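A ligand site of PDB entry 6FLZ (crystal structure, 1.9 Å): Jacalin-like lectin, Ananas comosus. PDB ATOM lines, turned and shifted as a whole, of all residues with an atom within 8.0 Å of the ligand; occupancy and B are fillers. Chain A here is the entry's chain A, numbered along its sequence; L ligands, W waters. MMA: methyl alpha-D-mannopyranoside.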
ATOM      1  N   ARG A  32      10.791  -9.222  15.830  1.00  0.00           N
ATOM      2  CA  ARG A  32      10.822  -7.873  15.297  1.00  0.00           C
ATOM      3  C   ARG A  32      10.512  -7.923  13.806  1.00  0.00           C
ATOM      4  O   ARG A  32      11.076  -8.750  13.080  1.00  0.00           O
ATOM      5  CB  ARG A  32      12.185  -7.214  15.524  1.00  0.00           C
ATOM      6  CG  ARG A  32      12.636  -7.136  16.971  1.00  0.00           C
ATOM      7  CD  ARG A  32      13.851  -6.224  17.104  1.00  0.00           C
ATOM      8  NE  ARG A  32      13.481  -4.862  16.725  1.00  0.00           N
ATOM      9  CZ  ARG A  32      12.955  -3.969  17.563  1.00  0.00           C
ATOM     10  NH1 ARG A  32      12.776  -4.267  18.843  1.00  0.00           N
ATOM     11  NH2 ARG A  32      12.622  -2.767  17.099  1.00  0.00           N
ATOM     12  N   SER A  33       9.604  -7.054  13.357  1.00  0.00           N
ATOM     13  CA  SER A  33       9.177  -7.140  11.963  1.00  0.00           C
ATOM     14  C   SER A  33       8.580  -5.834  11.500  1.00  0.00           C
ATOM     15  O   SER A  33       8.191  -4.975  12.309  1.00  0.00           O
ATOM     16  CB  SER A  33       8.157  -8.270  11.757  1.00  0.00           C
ATOM     17  OG  SER A  33       6.933  -7.963  12.395  1.00  0.00           O
ATOM     18  N   ALA A  34       8.505  -5.694  10.180  1.00  0.00           N
ATOM     19  CA  ALA A  34       7.801  -4.612   9.506  1.00  0.00           C
ATOM     20  C   ALA A  34       7.517  -5.060   8.072  1.00  0.00           C
ATOM     21  O   ALA A  34       6.559  -5.799   7.837  1.00  0.00           O
ATOM     22  CB  ALA A  34       8.621  -3.322   9.556  1.00  0.00           C
ATOM     23  N   HIS A  35       8.334  -4.645   7.103  1.00  0.00           N
ATOM     24  CA  HIS A  35       8.212  -5.159   5.741  1.00  0.00           C
ATOM     25  C   HIS A  35       8.850  -6.521   5.571  1.00  0.00           C
ATOM     26  O   HIS A  35       8.548  -7.223   4.586  1.00  0.00           O
ATOM     27  CB  HIS A  35       8.811  -4.154   4.754  1.00  0.00           C
ATOM     28  CG  HIS A  35       7.985  -2.922   4.592  1.00  0.00           C
ATOM     29  ND1 HIS A  35       7.647  -2.409   3.357  1.00  0.00           N
ATOM     30  CD2 HIS A  35       7.402  -2.108   5.507  1.00  0.00           C
ATOM     31  CE1 HIS A  35       6.903  -1.323   3.520  1.00  0.00           C
ATOM     32  NE2 HIS A  35       6.743  -1.126   4.811  1.00  0.00           N
ATOM     33  N   ALA A  36       9.740  -6.913   6.474  1.00  0.00           N
ATOM     34  CA  ALA A  36      10.297  -8.259   6.516  1.00  0.00           C
ATOM     35  C   ALA A  36      10.417  -8.649   7.986  1.00  0.00           C
ATOM     36  O   ALA A  36       9.932  -7.944   8.865  1.00  0.00           O
ATOM     37  CB  ALA A  36      11.638  -8.314   5.777  1.00  0.00           C
ATOM     38  N   ILE A  37      11.083  -9.777   8.246  1.00  0.00           N
ATOM     39  CA  ILE A  37      11.364 -10.186   9.623  1.00  0.00           C
ATOM     40  C   ILE A  37      12.746  -9.666   9.970  1.00  0.00           C
ATOM     41  O   ILE A  37      13.743 -10.055   9.349  1.00  0.00           O
ATOM     42  CB  ILE A  37      11.293 -11.710   9.796  1.00  0.00           C
ATOM     43  CG1 ILE A  37       9.937 -12.261   9.328  1.00  0.00           C
ATOM     44  CG2 ILE A  37      11.527 -12.083  11.264  1.00  0.00           C
ATOM     45  CD1 ILE A  37       8.715 -11.529   9.894  1.00  0.00           C
ATOM     46  N   ASP A  38      12.806  -8.793  10.978  1.00  0.00           N
ATOM     47  CA  ASP A  38      14.051  -8.159  11.396  1.00  0.00           C
ATOM     48  C   ASP A  38      14.846  -9.011  12.376  1.00  0.00           C
ATOM     49  O   ASP A  38      16.084  -9.040  12.296  1.00  0.00           O
ATOM     50  CB  ASP A  38      13.763  -6.789  12.020  1.00  0.00           C
ATOM     51  CG  ASP A  38      13.356  -5.752  10.995  1.00  0.00           C
ATOM     52  OD1 ASP A  38      12.160  -5.698  10.635  1.00  0.00           O
ATOM     53  OD2 ASP A  38      14.234  -4.987  10.533  1.00  0.00           O
ATOM     54  N   ALA A  39      14.193  -9.665  13.333  1.00  0.00           N
ATOM     55  CA  ALA A  39      14.912 -10.393  14.368  1.00  0.00           C
ATOM     56  C   ALA A  39      14.012 -11.432  15.028  1.00  0.00           C
ATOM     57  O   ALA A  39      12.789 -11.301  15.053  1.00  0.00           O
ATOM     58  CB  ALA A  39      15.471  -9.443  15.430  1.00  0.00           C
ATOM     59  N   GLY A  58      18.615  -7.814  13.566  1.00  0.00           N
ATOM     60  CA  GLY A  58      18.822  -6.413  13.856  1.00  0.00           C
ATOM     61  C   GLY A  58      17.733  -5.806  14.732  1.00  0.00           C
ATOM     62  O   GLY A  58      16.856  -6.489  15.251  1.00  0.00           O
ATOM     63  N   ASN A  59      17.811  -4.478  14.884  1.00  0.00           N
ATOM     64  CA  ASN A  59      16.916  -3.740  15.758  1.00  0.00           C
ATOM     65  C   ASN A  59      15.887  -2.909  14.990  1.00  0.00           C
ATOM     66  O   ASN A  59      15.265  -2.009  15.567  1.00  0.00           O
ATOM     67  CB  ASN A  59      17.725  -2.835  16.682  1.00  0.00           C
ATOM     68  CG  ASN A  59      18.439  -3.635  17.753  1.00  0.00           C
ATOM     69  OD1 ASN A  59      17.871  -4.551  18.335  1.00  0.00           O
ATOM     70  ND2 ASN A  59      19.707  -3.311  17.986  1.00  0.00           N
ATOM     71  N   GLY A  60      15.683  -3.209  13.709  1.00  0.00           N
ATOM     72  CA  GLY A  60      14.655  -2.552  12.940  1.00  0.00           C
ATOM     73  C   GLY A  60      13.272  -3.109  13.227  1.00  0.00           C
ATOM     74  O   GLY A  60      13.071  -4.007  14.056  1.00  0.00           O
ATOM     75  N   GLY A  61      12.293  -2.545  12.523  1.00  0.00           N
ATOM     76  CA  GLY A  61      10.893  -2.924  12.668  1.00  0.00           C
ATOM     77  C   GLY A  61      10.338  -2.632  14.058  1.00  0.00           C
ATOM     78  O   GLY A  61      10.864  -1.821  14.816  1.00  0.00           O
ATOM     79  N   LYS A  62       9.222  -3.299  14.351  1.00  0.00           N
ATOM     80  CA  LYS A  62       8.566  -3.211  15.644  1.00  0.00           C
ATOM     81  C   LYS A  62       8.526  -4.606  16.278  1.00  0.00           C
ATOM     82  O   LYS A  62       8.532  -5.622  15.590  1.00  0.00           O
ATOM     83  CB  LYS A  62       7.141  -2.667  15.499  1.00  0.00           C
ATOM     84  CG  LYS A  62       6.165  -3.655  14.873  1.00  0.00           C
ATOM     85  CD  LYS A  62       4.758  -3.076  14.766  1.00  0.00           C
ATOM     86  CE  LYS A  62       3.719  -4.134  15.075  1.00  0.00           C
ATOM     87  NZ  LYS A  62       3.622  -4.402  16.543  1.00  0.00           N
ATOM     88  N   LEU A  84      14.424  -8.411  -0.893  1.00  0.00           N
ATOM     89  CA  LEU A  84      14.055  -7.099  -0.372  1.00  0.00           C
ATOM     90  C   LEU A  84      15.274  -6.191  -0.453  1.00  0.00           C
ATOM     91  O   LEU A  84      16.345  -6.550   0.062  1.00  0.00           O
ATOM     92  CB  LEU A  84      13.534  -7.189   1.057  1.00  0.00           C
ATOM     93  CG  LEU A  84      13.041  -5.849   1.595  1.00  0.00           C
ATOM     94  CD1 LEU A  84      11.756  -5.443   0.886  1.00  0.00           C
ATOM     95  CD2 LEU A  84      12.795  -5.930   3.091  1.00  0.00           C
ATOM     96  N   LEU A  90      15.502 -13.312   1.634  1.00  0.00           N
ATOM     97  CA  LEU A  90      15.402 -13.297   3.088  1.00  0.00           C
ATOM     98  C   LEU A  90      13.974 -13.647   3.491  1.00  0.00           C
ATOM     99  O   LEU A  90      13.112 -13.906   2.656  1.00  0.00           O
ATOM    100  CB  LEU A  90      15.869 -11.953   3.671  1.00  0.00           C
ATOM    101  CG  LEU A  90      15.286 -10.618   3.158  1.00  0.00           C
ATOM    102  CD1 LEU A  90      13.777 -10.547   3.283  1.00  0.00           C
ATOM    103  CD2 LEU A  90      15.926  -9.440   3.901  1.00  0.00           C
ATOM    104  N   VAL A  91      13.724 -13.655   4.804  1.00  0.00           N
ATOM    105  CA  VAL A  91      12.419 -14.054   5.337  1.00  0.00           C
ATOM    106  C   VAL A  91      11.530 -12.815   5.400  1.00  0.00           C
ATOM    107  O   VAL A  91      11.804 -11.886   6.166  1.00  0.00           O
ATOM    108  CB  VAL A  91      12.541 -14.734   6.704  1.00  0.00           C
ATOM    109  CG1 VAL A  91      11.165 -15.193   7.199  1.00  0.00           C
ATOM    110  CG2 VAL A  91      13.500 -15.911   6.626  1.00  0.00           C
ATOM    111  N   ARG A  92      10.471 -12.814   4.594  1.00  0.00           N
ATOM    112  CA  ARG A  92       9.574 -11.669   4.495  1.00  0.00           C
ATOM    113  C   ARG A  92       8.460 -11.704   5.538  1.00  0.00           C
ATOM    114  O   ARG A  92       8.029 -10.639   6.004  1.00  0.00           O
ATOM    115  CB  ARG A  92       8.913 -11.620   3.103  1.00  0.00           C
ATOM    116  CG  ARG A  92       9.821 -11.240   1.943  1.00  0.00           C
ATOM    117  CD  ARG A  92      10.486  -9.880   2.117  1.00  0.00           C
ATOM    118  NE  ARG A  92       9.535  -8.787   2.339  1.00  0.00           N
ATOM    119  CZ  ARG A  92       8.910  -8.114   1.385  1.00  0.00           C
ATOM    120  NH1 ARG A  92       9.102  -8.400   0.100  1.00  0.00           N
ATOM    121  NH2 ARG A  92       8.070  -7.128   1.706  1.00  0.00           N
ATOM    122  N   GLY A 107       5.583  -9.257   9.439  1.00  0.00           N
ATOM    123  CA  GLY A 107       6.187  -8.912   8.173  1.00  0.00           C
ATOM    124  C   GLY A 107       5.123  -8.684   7.111  1.00  0.00           C
ATOM    125  O   GLY A 107       3.991  -8.287   7.403  1.00  0.00           O
ATOM    126  N   LEU A 108       5.479  -8.959   5.855  1.00  0.00           N
ATOM    127  CA  LEU A 108       4.569  -8.846   4.728  1.00  0.00           C
ATOM    128  C   LEU A 108       4.604 -10.146   3.932  1.00  0.00           C
ATOM    129  O   LEU A 108       5.694 -10.636   3.589  1.00  0.00           O
ATOM    130  CB  LEU A 108       4.934  -7.663   3.822  1.00  0.00           C
ATOM    131  CG  LEU A 108       4.651  -6.259   4.348  1.00  0.00           C
ATOM    132  CD1 LEU A 108       5.199  -5.210   3.391  1.00  0.00           C
ATOM    133  CD2 LEU A 108       3.166  -6.057   4.565  1.00  0.00           C
ATOM    134  N   SER A 132      21.412  -7.842   9.518  1.00  0.00           N
ATOM    135  CA  SER A 132      20.478  -6.825   9.960  1.00  0.00           C
ATOM    136  C   SER A 132      19.046  -7.361  10.020  1.00  0.00           C
ATOM    137  O   SER A 132      18.227  -6.820  10.760  1.00  0.00           O
ATOM    138  CB  SER A 132      20.511  -5.614   9.012  1.00  0.00           C
ATOM    139  OG  SER A 132      21.822  -5.085   8.924  1.00  0.00           O
ATOM    140  N   LEU A 133      18.748  -8.402   9.235  1.00  0.00           N
ATOM    141  CA  LEU A 133      17.422  -9.001   9.157  1.00  0.00           C
ATOM    142  C   LEU A 133      17.564 -10.510   9.301  1.00  0.00           C
ATOM    143  O   LEU A 133      18.660 -11.044   9.486  1.00  0.00           O
ATOM    144  CB  LEU A 133      16.724  -8.630   7.841  1.00  0.00           C
ATOM    145  CG  LEU A 133      16.585  -7.135   7.504  1.00  0.00           C
ATOM    146  CD1 LEU A 133      16.073  -6.943   6.082  1.00  0.00           C
ATOM    147  CD2 LEU A 133      15.634  -6.445   8.454  1.00  0.00           C
HETATM  148  C1  MMA L   1      10.883  -0.909   7.546  1.00  0.00           C
HETATM  149  C2  MMA L   1      11.568  -0.425   8.814  1.00  0.00           C
HETATM  150  C3  MMA L   1      12.913  -1.020   8.973  1.00  0.00           C
HETATM  151  C4  MMA L   1      12.896  -2.521   8.825  1.00  0.00           C
HETATM  152  C5  MMA L   1      12.290  -2.952   7.489  1.00  0.00           C
HETATM  153  C6  MMA L   1      12.296  -4.465   7.378  1.00  0.00           C
HETATM  154  C7  MMA L   1      11.034  -0.622   5.228  1.00  0.00           C
HETATM  155  O1  MMA L   1      11.539  -0.315   6.508  1.00  0.00           O
HETATM  156  O2  MMA L   1      10.768  -0.731   9.982  1.00  0.00           O
HETATM  157  O3  MMA L   1      13.416  -0.659  10.287  1.00  0.00           O
HETATM  158  O4  MMA L   1      14.232  -2.993   8.901  1.00  0.00           O
HETATM  159  O5  MMA L   1      10.923  -2.416   7.371  1.00  0.00           O
HETATM  160  O6  MMA L   1      11.303  -5.032   8.197  1.00  0.00           O
HETATM  161  O   HOH W   1      16.231  -0.834  10.004  1.00  0.00           O
HETATM  162  O   HOH W   2       8.539   0.892  10.407  1.00  0.00           O
HETATM  163  O   HOH W   3      12.484  -1.894   2.987  1.00  0.00           O
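O of Ala 36 lies within hydrogen-bond range of O6 of the ligand, 3.3 Å away.
The side-chain carboxylate of Asp 38 lies within hydrogen-bond range of an oxygen (O4) of the ligand, 2.6 Å away.
An oxygen (O6) of the ligand lies close to the backbone NH of Ala 34.
N of His 35 is in hydrogen-bond range of O6 of the ligand (3.2 Å).
N of Gly 61 is in hydrogen-bond range of O3 of the ligand (3.1 Å).
The backbone NH (N) of Ala 36 lies within hydrogen-bond range of an oxygen (O6) of the ligand (3.0 Å).
Gly 60 touches the ligand.
Leu 133 touches the ligand (CD2 to O4, 3.8 Å).
Hydrophobic or aromatic side chains that line the ligand: Ala 34, His 35 and Leu 133.
Within 4 Å of the ligand: Ala 34, His 35, Ala 36, Asp 38, Gly 60, Gly 61 and Leu 133.
The nearest printed residue that does not touch the ligand is Ser 33 (4.4 Å).
The backbone NH (N) of Asp 38 lies within hydrogen-bond range of the backbone carbonyl oxygen (O) of Arg 32 (2.7 Å).
N of Gly 58 is in hydrogen-bond range of O of Asp 38 (3.1 Å).
The guanidinium group (NH2) of Arg 32 sits at hydrogen-bond distance from the backbone carbonyl oxygen (O) of Gly 61.
The backbone carbonyl oxygen (O) of His 35 lies within hydrogen-bond range of the guanidinium group (NE) of Arg 92 (2.9 Å).
NE of Arg 32 lies within hydrogen-bond range of O of Gly 60 (2.8 Å).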
